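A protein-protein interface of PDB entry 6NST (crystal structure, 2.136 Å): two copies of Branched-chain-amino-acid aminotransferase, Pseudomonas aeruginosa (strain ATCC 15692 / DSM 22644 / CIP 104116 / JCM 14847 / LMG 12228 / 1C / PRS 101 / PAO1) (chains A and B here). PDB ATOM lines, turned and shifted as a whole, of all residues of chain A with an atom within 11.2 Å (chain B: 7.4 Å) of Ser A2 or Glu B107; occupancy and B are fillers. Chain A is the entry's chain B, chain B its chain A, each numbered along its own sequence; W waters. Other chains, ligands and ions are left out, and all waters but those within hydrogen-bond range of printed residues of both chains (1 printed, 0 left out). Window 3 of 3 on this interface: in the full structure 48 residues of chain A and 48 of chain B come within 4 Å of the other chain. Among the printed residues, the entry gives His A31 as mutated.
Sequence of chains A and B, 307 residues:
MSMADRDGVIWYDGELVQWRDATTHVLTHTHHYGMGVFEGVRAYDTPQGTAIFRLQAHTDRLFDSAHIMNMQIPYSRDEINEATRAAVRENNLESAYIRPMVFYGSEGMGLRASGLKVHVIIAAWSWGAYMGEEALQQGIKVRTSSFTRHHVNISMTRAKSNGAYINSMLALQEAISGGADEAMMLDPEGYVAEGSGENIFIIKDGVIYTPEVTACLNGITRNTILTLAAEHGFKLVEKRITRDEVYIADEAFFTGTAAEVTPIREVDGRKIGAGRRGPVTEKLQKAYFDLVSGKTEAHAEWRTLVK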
ATOM      1  N   SER A   2      10.904  26.873  -8.062  1.00  0.00           N
ATOM      2  CA  SER A   2      10.187  26.398  -9.239  1.00  0.00           C
ATOM      3  C   SER A   2       9.115  25.378  -8.865  1.00  0.00           C
ATOM      4  O   SER A   2       9.316  24.544  -7.981  1.00  0.00           O
ATOM      5  CB  SER A   2      11.159  25.786 -10.249  1.00  0.00           C
ATOM      6  OG  SER A   2      10.471  25.332 -11.403  1.00  0.00           O
ATOM      7  N   MET A   3       7.974  25.449  -9.549  1.00  0.00           N
ATOM      8  CA  MET A   3       6.853  24.552  -9.306  1.00  0.00           C
ATOM      9  C   MET A   3       6.791  23.399 -10.297  1.00  0.00           C
ATOM     10  O   MET A   3       5.878  22.571 -10.207  1.00  0.00           O
ATOM     11  CB  MET A   3       5.535  25.332  -9.342  1.00  0.00           C
ATOM     12  CG  MET A   3       4.619  25.025  -8.179  1.00  0.00           C
ATOM     13  SD  MET A   3       5.353  25.560  -6.625  1.00  0.00           S
ATOM     14  CE  MET A   3       4.669  24.355  -5.495  1.00  0.00           C
ATOM     15  N   ALA A   4       7.729  23.324 -11.234  1.00  0.00           N
ATOM     16  CA  ALA A   4       7.747  22.281 -12.252  1.00  0.00           C
ATOM     17  C   ALA A   4       8.933  21.342 -12.132  1.00  0.00           C
ATOM     18  O   ALA A   4       8.763  20.125 -12.253  1.00  0.00           O
ATOM     19  CB  ALA A   4       7.743  22.912 -13.652  1.00  0.00           C
ATOM     20  N   ASP A   5      10.135  21.872 -11.897  1.00  0.00           N
ATOM     21  CA  ASP A   5      11.349  21.059 -11.841  1.00  0.00           C
ATOM     22  C   ASP A   5      11.558  20.584 -10.404  1.00  0.00           C
ATOM     23  O   ASP A   5      12.400  21.088  -9.658  1.00  0.00           O
ATOM     24  CB  ASP A   5      12.546  21.850 -12.355  1.00  0.00           C
ATOM     25  CG  ASP A   5      13.790  20.997 -12.502  1.00  0.00           C
ATOM     26  OD1 ASP A   5      13.886  20.250 -13.498  1.00  0.00           O
ATOM     27  OD2 ASP A   5      14.672  21.071 -11.621  1.00  0.00           O
ATOM     28  N   ARG A   6      10.764  19.587 -10.018  1.00  0.00           N
ATOM     29  CA  ARG A   6      10.886  18.975  -8.704  1.00  0.00           C
ATOM     30  C   ARG A   6      10.378  17.544  -8.777  1.00  0.00           C
ATOM     31  O   ARG A   6       9.608  17.181  -9.671  1.00  0.00           O
ATOM     32  CB  ARG A   6      10.120  19.765  -7.634  1.00  0.00           C
ATOM     33  CG  ARG A   6       8.614  19.766  -7.813  1.00  0.00           C
ATOM     34  CD  ARG A   6       7.931  20.494  -6.666  1.00  0.00           C
ATOM     35  NE  ARG A   6       8.344  21.893  -6.583  1.00  0.00           N
ATOM     36  CZ  ARG A   6       8.028  22.704  -5.579  1.00  0.00           C
ATOM     37  NH1 ARG A   6       8.445  23.964  -5.586  1.00  0.00           N
ATOM     38  NH2 ARG A   6       7.299  22.257  -4.566  1.00  0.00           N
ATOM     39  N   ASP A   7      10.822  16.731  -7.823  1.00  0.00           N
ATOM     40  CA  ASP A   7      10.416  15.336  -7.770  1.00  0.00           C
ATOM     41  C   ASP A   7       9.010  15.207  -7.195  1.00  0.00           C
ATOM     42  O   ASP A   7       8.540  16.067  -6.444  1.00  0.00           O
ATOM     43  CB  ASP A   7      11.400  14.518  -6.931  1.00  0.00           C
ATOM     44  CG  ASP A   7      12.765  14.398  -7.583  1.00  0.00           C
ATOM     45  OD1 ASP A   7      12.831  14.343  -8.829  1.00  0.00           O
ATOM     46  OD2 ASP A   7      13.774  14.356  -6.847  1.00  0.00           O
ATOM     47  N   GLY A   8       8.340  14.119  -7.558  1.00  0.00           N
ATOM     48  CA  GLY A   8       6.993  13.876  -7.085  1.00  0.00           C
ATOM     49  C   GLY A   8       6.058  13.394  -8.173  1.00  0.00           C
ATOM     50  O   GLY A   8       6.453  13.284  -9.338  1.00  0.00           O
ATOM     51  N   ILE A  10       1.916  13.747  -9.806  1.00  0.00           N
ATOM     52  CA  ILE A  10       0.711  14.556  -9.904  1.00  0.00           C
ATOM     53  C   ILE A  10      -0.372  13.703 -10.543  1.00  0.00           C
ATOM     54  O   ILE A  10      -0.117  13.010 -11.536  1.00  0.00           O
ATOM     55  CB  ILE A  10       0.950  15.844 -10.717  1.00  0.00           C
ATOM     56  CG1 ILE A  10       1.871  16.795  -9.948  1.00  0.00           C
ATOM     57  CG2 ILE A  10      -0.367  16.527 -11.057  1.00  0.00           C
ATOM     58  CD1 ILE A  10       2.275  18.031 -10.725  1.00  0.00           C
ATOM     59  N   TRP A  19       6.072  14.448 -11.799  1.00  0.00           N
ATOM     60  CA  TRP A  19       5.822  15.875 -11.613  1.00  0.00           C
ATOM     61  C   TRP A  19       6.301  16.684 -12.811  1.00  0.00           C
ATOM     62  O   TRP A  19       5.598  17.585 -13.285  1.00  0.00           O
ATOM     63  CB  TRP A  19       6.502  16.364 -10.332  1.00  0.00           C
ATOM     64  CG  TRP A  19       6.064  17.734  -9.887  1.00  0.00           C
ATOM     65  CD1 TRP A  19       6.385  18.930 -10.465  1.00  0.00           C
ATOM     66  CD2 TRP A  19       5.233  18.044  -8.760  1.00  0.00           C
ATOM     67  NE1 TRP A  19       5.800  19.963  -9.770  1.00  0.00           N
ATOM     68  CE2 TRP A  19       5.089  19.446  -8.719  1.00  0.00           C
ATOM     69  CE3 TRP A  19       4.596  17.271  -7.784  1.00  0.00           C
ATOM     70  CZ2 TRP A  19       4.334  20.090  -7.741  1.00  0.00           C
ATOM     71  CZ3 TRP A  19       3.845  17.914  -6.815  1.00  0.00           C
ATOM     72  CH2 TRP A  19       3.722  19.308  -6.799  1.00  0.00           C
ATOM     73  N   ARG A  20       7.498  16.378 -13.316  1.00  0.00           N
ATOM     74  CA  ARG A  20       8.023  17.100 -14.468  1.00  0.00           C
ATOM     75  C   ARG A  20       7.329  16.707 -15.763  1.00  0.00           C
ATOM     76  O   ARG A  20       7.400  17.458 -16.742  1.00  0.00           O
ATOM     77  CB  ARG A  20       9.530  16.867 -14.588  1.00  0.00           C
ATOM     78  CG  ARG A  20      10.310  17.320 -13.367  1.00  0.00           C
ATOM     79  CD  ARG A  20      11.789  17.009 -13.498  1.00  0.00           C
ATOM     80  NE  ARG A  20      12.535  17.474 -12.332  1.00  0.00           N
ATOM     81  CZ  ARG A  20      12.728  16.752 -11.234  1.00  0.00           C
ATOM     82  NH1 ARG A  20      12.233  15.523 -11.148  1.00  0.00           N
ATOM     83  NH2 ARG A  20      13.417  17.257 -10.219  1.00  0.00           N
ATOM     84  N   ALA A  22       4.009  16.218 -15.901  1.00  0.00           N
ATOM     85  CA  ALA A  22       2.649  16.754 -15.845  1.00  0.00           C
ATOM     86  C   ALA A  22       2.630  18.081 -16.600  1.00  0.00           C
ATOM     87  O   ALA A  22       2.710  19.170 -16.025  1.00  0.00           O
ATOM     88  CB  ALA A  22       2.189  16.920 -14.403  1.00  0.00           C
ATOM     89  N   HIS A  31      -5.733  28.140 -20.409  1.00  0.00           N
ATOM     90  CA  HIS A  31      -4.581  29.024 -20.283  1.00  0.00           C
ATOM     91  C   HIS A  31      -4.833  30.366 -20.956  1.00  0.00           C
ATOM     92  O   HIS A  31      -4.407  31.407 -20.447  1.00  0.00           O
ATOM     93  CB  HIS A  31      -3.352  28.342 -20.884  1.00  0.00           C
ATOM     94  CG  HIS A  31      -2.050  28.860 -20.365  1.00  0.00           C
ATOM     95  ND1 HIS A  31      -0.849  28.230 -20.612  1.00  0.00           N
ATOM     96  CD2 HIS A  31      -1.760  29.944 -19.610  1.00  0.00           C
ATOM     97  CE1 HIS A  31       0.125  28.906 -20.031  1.00  0.00           C
ATOM     98  NE2 HIS A  31      -0.400  29.950 -19.417  1.00  0.00           N
ATOM     99  N   ALA A 123      -2.373  18.390  -7.715  1.00  0.00           N
ATOM    100  CA  ALA A 123      -0.982  18.462  -7.296  1.00  0.00           C
ATOM    101  C   ALA A 123      -0.908  18.832  -5.822  1.00  0.00           C
ATOM    102  O   ALA A 123      -1.663  19.686  -5.346  1.00  0.00           O
ATOM    103  CB  ALA A 123      -0.204  19.483  -8.132  1.00  0.00           C
ATOM    104  N   ALA A 124       0.005  18.185  -5.102  1.00  0.00           N
ATOM    105  CA  ALA A 124       0.195  18.424  -3.680  1.00  0.00           C
ATOM    106  C   ALA A 124       1.676  18.610  -3.386  1.00  0.00           C
ATOM    107  O   ALA A 124       2.518  17.866  -3.896  1.00  0.00           O
ATOM    108  CB  ALA A 124      -0.366  17.271  -2.837  1.00  0.00           C
ATOM    109  N   TRP A 125       1.985  19.607  -2.559  1.00  0.00           N
ATOM    110  CA  TRP A 125       3.358  19.903  -2.178  1.00  0.00           C
ATOM    111  C   TRP A 125       3.390  20.360  -0.729  1.00  0.00           C
ATOM    112  O   TRP A 125       2.409  20.897  -0.208  1.00  0.00           O
ATOM    113  CB  TRP A 125       3.980  20.974  -3.082  1.00  0.00           C
ATOM    114  CG  TRP A 125       3.194  22.244  -3.138  1.00  0.00           C
ATOM    115  CD1 TRP A 125       3.338  23.335  -2.332  1.00  0.00           C
ATOM    116  CD2 TRP A 125       2.141  22.559  -4.056  1.00  0.00           C
ATOM    117  NE1 TRP A 125       2.438  24.310  -2.691  1.00  0.00           N
ATOM    118  CE2 TRP A 125       1.691  23.858  -3.748  1.00  0.00           C
ATOM    119  CE3 TRP A 125       1.535  21.868  -5.111  1.00  0.00           C
ATOM    120  CZ2 TRP A 125       0.666  24.480  -4.455  1.00  0.00           C
ATOM    121  CZ3 TRP A 125       0.516  22.487  -5.812  1.00  0.00           C
ATOM    122  CH2 TRP A 125       0.092  23.780  -5.480  1.00  0.00           C
ATOM    123  N   SER A 126       4.538  20.147  -0.088  1.00  0.00           N
ATOM    124  CA  SER A 126       4.677  20.416   1.334  1.00  0.00           C
ATOM    125  C   SER A 126       4.467  21.898   1.635  1.00  0.00           C
ATOM    126  O   SER A 126       4.610  22.767   0.771  1.00  0.00           O
ATOM    127  CB  SER A 126       6.054  19.972   1.827  1.00  0.00           C
ATOM    128  OG  SER A 126       6.214  20.254   3.205  1.00  0.00           O
ATOM    129  N   LEU B  27       1.096  23.255 -13.724  1.00  0.00           N
ATOM    130  CA  LEU B  27       1.016  24.239 -12.652  1.00  0.00           C
ATOM    131  C   LEU B  27       1.444  25.629 -13.106  1.00  0.00           C
ATOM    132  O   LEU B  27       1.930  26.425 -12.289  1.00  0.00           O
ATOM    133  CB  LEU B  27       1.852  23.785 -11.456  1.00  0.00           C
ATOM    134  CG  LEU B  27       1.342  22.523 -10.764  1.00  0.00           C
ATOM    135  CD1 LEU B  27       2.178  22.214  -9.535  1.00  0.00           C
ATOM    136  CD2 LEU B  27      -0.125  22.681 -10.397  1.00  0.00           C
ATOM    137  N   THR B  28       1.287  25.935 -14.392  1.00  0.00           N
ATOM    138  CA  THR B  28       1.563  27.273 -14.896  1.00  0.00           C
ATOM    139  C   THR B  28       0.662  28.293 -14.207  1.00  0.00           C
ATOM    140  O   THR B  28      -0.533  28.057 -14.012  1.00  0.00           O
ATOM    141  CB  THR B  28       1.355  27.308 -16.412  1.00  0.00           C
ATOM    142  OG1 THR B  28       2.161  26.296 -17.028  1.00  0.00           O
ATOM    143  CG2 THR B  28       1.741  28.654 -16.977  1.00  0.00           C
ATOM    144  N   HIS B  29       1.247  29.437 -13.837  1.00  0.00           N
ATOM    145  CA  HIS B  29       0.536  30.410 -13.011  1.00  0.00           C
ATOM    146  C   HIS B  29      -0.645  31.025 -13.759  1.00  0.00           C
ATOM    147  O   HIS B  29      -1.754  31.119 -13.218  1.00  0.00           O
ATOM    148  CB  HIS B  29       1.502  31.496 -12.538  1.00  0.00           C
ATOM    149  CG  HIS B  29       0.960  32.353 -11.438  1.00  0.00           C
ATOM    150  ND1 HIS B  29       0.156  33.448 -11.674  1.00  0.00           N
ATOM    151  CD2 HIS B  29       1.114  32.283 -10.094  1.00  0.00           C
ATOM    152  CE1 HIS B  29      -0.162  34.014 -10.524  1.00  0.00           C
ATOM    153  NE2 HIS B  29       0.406  33.327  -9.549  1.00  0.00           N
ATOM    154  N   PHE B 103       2.496  35.047 -20.650  1.00  0.00           N
ATOM    155  CA  PHE B 103       1.954  34.381 -19.473  1.00  0.00           C
ATOM    156  C   PHE B 103       3.047  34.137 -18.441  1.00  0.00           C
ATOM    157  O   PHE B 103       4.225  34.000 -18.778  1.00  0.00           O
ATOM    158  CB  PHE B 103       1.264  33.054 -19.837  1.00  0.00           C
ATOM    159  CG  PHE B 103       2.194  31.994 -20.370  1.00  0.00           C
ATOM    160  CD1 PHE B 103       2.705  31.014 -19.532  1.00  0.00           C
ATOM    161  CD2 PHE B 103       2.532  31.958 -21.714  1.00  0.00           C
ATOM    162  CE1 PHE B 103       3.546  30.030 -20.020  1.00  0.00           C
ATOM    163  CE2 PHE B 103       3.373  30.977 -22.209  1.00  0.00           C
ATOM    164  CZ  PHE B 103       3.880  30.010 -21.360  1.00  0.00           C
ATOM    165  N   TYR B 104       2.634  34.088 -17.174  1.00  0.00           N
ATOM    166  CA  TYR B 104       3.539  33.749 -16.086  1.00  0.00           C
ATOM    167  C   TYR B 104       3.812  32.250 -16.074  1.00  0.00           C
ATOM    168  O   TYR B 104       2.936  31.440 -16.371  1.00  0.00           O
ATOM    169  CB  TYR B 104       2.949  34.177 -14.741  1.00  0.00           C
ATOM    170  CG  TYR B 104       3.086  35.651 -14.436  1.00  0.00           C
ATOM    171  CD1 TYR B 104       4.249  36.343 -14.751  1.00  0.00           C
ATOM    172  CD2 TYR B 104       2.049  36.353 -13.832  1.00  0.00           C
ATOM    173  CE1 TYR B 104       4.376  37.693 -14.470  1.00  0.00           C
ATOM    174  CE2 TYR B 104       2.167  37.701 -13.548  1.00  0.00           C
ATOM    175  CZ  TYR B 104       3.330  38.366 -13.870  1.00  0.00           C
ATOM    176  OH  TYR B 104       3.451  39.708 -13.590  1.00  0.00           O
ATOM    177  N   GLY B 105       5.040  31.885 -15.712  1.00  0.00           N
ATOM    178  CA  GLY B 105       5.468  30.503 -15.754  1.00  0.00           C
ATOM    179  C   GLY B 105       5.054  29.721 -14.523  1.00  0.00           C
ATOM    180  O   GLY B 105       4.207  30.146 -13.734  1.00  0.00           O
ATOM    181  N   SER B 106       5.677  28.553 -14.360  1.00  0.00           N
ATOM    182  CA  SER B 106       5.398  27.692 -13.216  1.00  0.00           C
ATOM    183  C   SER B 106       6.454  27.822 -12.121  1.00  0.00           C
ATOM    184  O   SER B 106       7.063  26.825 -11.712  1.00  0.00           O
ATOM    185  CB  SER B 106       5.274  26.243 -13.681  1.00  0.00           C
ATOM    186  OG  SER B 106       6.406  25.860 -14.430  1.00  0.00           O
ATOM    187  N   GLU B 107       6.672  29.043 -11.631  1.00  0.00           N
ATOM    188  CA  GLU B 107       7.657  29.275 -10.578  1.00  0.00           C
ATOM    189  C   GLU B 107       7.025  29.264  -9.189  1.00  0.00           C
ATOM    190  O   GLU B 107       7.448  28.499  -8.315  1.00  0.00           O
ATOM    191  CB  GLU B 107       8.395  30.594 -10.828  1.00  0.00           C
ATOM    192  CG  GLU B 107       9.503  30.501 -11.865  1.00  0.00           C
ATOM    193  CD  GLU B 107       8.970  30.234 -13.255  1.00  0.00           C
ATOM    194  OE1 GLU B 107       7.849  30.696 -13.554  1.00  0.00           O
ATOM    195  OE2 GLU B 107       9.663  29.559 -14.046  1.00  0.00           O
ATOM    196  N   GLY B 108       6.011  30.100  -8.974  1.00  0.00           N
ATOM    197  CA  GLY B 108       5.287  30.150  -7.728  1.00  0.00           C
ATOM    198  C   GLY B 108       3.839  29.715  -7.894  1.00  0.00           C
ATOM    199  O   GLY B 108       3.375  29.367  -8.979  1.00  0.00           O
ATOM    200  N   MET B 109       3.122  29.741  -6.768  1.00  0.00           N
ATOM    201  CA  MET B 109       1.724  29.334  -6.766  1.00  0.00           C
ATOM    202  C   MET B 109       0.830  30.228  -5.915  1.00  0.00           C
ATOM    203  O   MET B 109      -0.370  29.949  -5.809  1.00  0.00           O
ATOM    204  CB  MET B 109       1.591  27.878  -6.290  1.00  0.00           C
ATOM    205  CG  MET B 109       0.448  27.119  -6.943  1.00  0.00           C
ATOM    206  SD  MET B 109       0.508  27.204  -8.744  1.00  0.00           S
ATOM    207  CE  MET B 109      -0.944  26.249  -9.169  1.00  0.00           C
ATOM    208  N   GLY B 110       1.375  31.291  -5.304  1.00  0.00           N
ATOM    209  CA  GLY B 110       0.567  32.230  -4.555  1.00  0.00           C
ATOM    210  C   GLY B 110       0.136  33.415  -5.402  1.00  0.00           C
ATOM    211  O   GLY B 110       0.631  33.639  -6.505  1.00  0.00           O
ATOM    212  N   GLY B 115       8.173  35.950  -7.630  1.00  0.00           N
ATOM    213  CA  GLY B 115       9.288  35.396  -8.372  1.00  0.00           C
ATOM    214  C   GLY B 115       8.838  34.669  -9.622  1.00  0.00           C
ATOM    215  O   GLY B 115       9.420  33.650 -10.005  1.00  0.00           O
ATOM    216  N   LEU B 116       7.799  35.192 -10.266  1.00  0.00           N
ATOM    217  CA  LEU B 116       7.229  34.551 -11.441  1.00  0.00           C
ATOM    218  C   LEU B 116       7.994  34.943 -12.695  1.00  0.00           C
ATOM    219  O   LEU B 116       8.317  36.116 -12.905  1.00  0.00           O
ATOM    220  CB  LEU B 116       5.754  34.928 -11.590  1.00  0.00           C
ATOM    221  CG  LEU B 116       4.825  34.446 -10.477  1.00  0.00           C
ATOM    222  CD1 LEU B 116       3.408  34.948 -10.702  1.00  0.00           C
ATOM    223  CD2 LEU B 116       4.852  32.929 -10.390  1.00  0.00           C
ATOM    224  N   LYS B 117       8.281  33.953 -13.534  1.00  0.00           N
ATOM    225  CA  LYS B 117       8.937  34.189 -14.809  1.00  0.00           C
ATOM    226  C   LYS B 117       7.894  34.408 -15.896  1.00  0.00           C
ATOM    227  O   LYS B 117       6.850  33.751 -15.918  1.00  0.00           O
ATOM    228  CB  LYS B 117       9.847  33.016 -15.179  1.00  0.00           C
ATOM    229  CG  LYS B 117      10.735  33.271 -16.385  1.00  0.00           C
ATOM    230  CD  LYS B 117      11.666  32.095 -16.639  1.00  0.00           C
ATOM    231  CE  LYS B 117      12.565  32.342 -17.839  1.00  0.00           C
ATOM    232  NZ  LYS B 117      11.776  32.545 -19.087  1.00  0.00           N
ATOM    233  N   VAL B 118       8.181  35.346 -16.792  1.00  0.00           N
ATOM    234  CA  VAL B 118       7.298  35.676 -17.903  1.00  0.00           C
ATOM    235  C   VAL B 118       7.736  34.886 -19.126  1.00  0.00           C
ATOM    236  O   VAL B 118       8.906  34.942 -19.527  1.00  0.00           O
ATOM    237  CB  VAL B 118       7.313  37.187 -18.194  1.00  0.00           C
ATOM    238  CG1 VAL B 118       6.415  37.503 -19.370  1.00  0.00           C
ATOM    239  CG2 VAL B 118       6.882  37.971 -16.964  1.00  0.00           C
ATOM    240  N   HIS B 119       6.800  34.145 -19.715  1.00  0.00           N
ATOM    241  CA  HIS B 119       7.026  33.400 -20.943  1.00  0.00           C
ATOM    242  C   HIS B 119       6.175  33.985 -22.061  1.00  0.00           C
ATOM    243  O   HIS B 119       5.116  34.568 -21.814  1.00  0.00           O
ATOM    244  CB  HIS B 119       6.694  31.917 -20.761  1.00  0.00           C
ATOM    245  CG  HIS B 119       7.496  31.246 -19.689  1.00  0.00           C
ATOM    246  ND1 HIS B 119       8.477  30.319 -19.963  1.00  0.00           N
ATOM    247  CD2 HIS B 119       7.463  31.371 -18.341  1.00  0.00           C
ATOM    248  CE1 HIS B 119       9.013  29.900 -18.831  1.00  0.00           C
ATOM    249  NE2 HIS B 119       8.416  30.522 -17.831  1.00  0.00           N
HETATM  250  O   HOH W   1       9.499  26.259 -13.988  1.00  0.00           O
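Ser A2 touches Ser B106 (OG to O, 3.7 Å).
CA of Ser A2 touches O of Glu B107, at 3.6 Å.
Leu B27 touches Met A3 (CD1 to O, 3.8 Å).
OG of Ser B106 touches CB of Ala A4, 3.3 Å away.
Leu B27 touches Trp A19.
Thr B28 touches His A31 (CG2 to CE1, 3.5 Å).
Phe B103 touches His A31 (CD1 to NE2, 3.3 Å).
CB of Ala A123 touches CD1 of Leu B27 (3.9 Å).
CZ2 of Trp A125 touches CG of Met B109, at 3.6 Å.
The backbone carbonyl oxygen (O) of Glu B107 is in hydrogen-bond range of the backbone NH (N) of Met A3 (3.3 Å).
O of Ser B106 is in hydrogen-bond range of N of Met A3, 2.7 Å away.
Printed residues of chain B that touch a printed residue of chain A: Leu B27, Thr B28, Phe B103, Ser B106, Glu B107 and Met B109.
Hydrophobic or aromatic side chains of chain B that line the printed part of chain A: Leu B27, Phe B103 and Met B109.
Of the 16 printed residues of chain A, 7 touch a printed residue of chain B.
Printed residues of chain A that touch a printed residue of chain B: Ser A2, Met A3, Ala A4, Trp A19, His A31, Ala A123 and Trp A125.
Hydrophobic or aromatic side chains of chain A that line the printed part of chain B: Met A3, Ala A4, Trp A19, His A31, Ala A123 and Trp A125.
Among the printed residues, 11 pairs touch across the chains.
The backbone carbonyl oxygen of Phe B103 lies within hydrogen-bond range of the backbone NH of His B119 (2.7 Å).
The guanidinium group of Arg A6 is in hydrogen-bond range of the backbone carbonyl oxygen of Ser A2 (2.6 Å).
N of Lys B117 is in hydrogen-bond range of OE1 of Glu B107 (3.3 Å).
SD of Met A3 lies within hydrogen-bond range of NH1 of Arg A6, 3.6 Å away.
O of Met A3 is in hydrogen-bond range of NE1 of Trp A19.
The side-chain hydroxyl (OG) of Ser A2 lies within hydrogen-bond range of the backbone NH (N) of Ala A4, at 3.4 Å.
No position is printed for both chains.
Ser A2 touches two residues of chain B.
Glu B107 touches two residues of chain A.
No residue of chain A comes within 4 Å of Gly B105.
Ser B106 touches three residues of chain A.
No residue of chain A comes within 4 Å of Lys B117.
Printed residues of chain A within 4 Å of Met B109: Trp A125 (3.6 Å).
Of the printed residues of chain A, Phe B103 touches His A31.
Printed residues of chain B within 4 Å of Ala A123: Leu B27 (3.9 Å).
Ile A10 touches none of the printed residues of chain B.
His B119 touches none of the printed residues of chain A.
Water W1 lies within hydrogen-bond range of the side-chain hydroxyl (OG) of Ser A2 (2.9 Å), the side-chain hydroxyl (OG) of Ser B106 (3.1 Å) and the side-chain carboxylate (OE2) of Glu B107 (3.3 Å).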
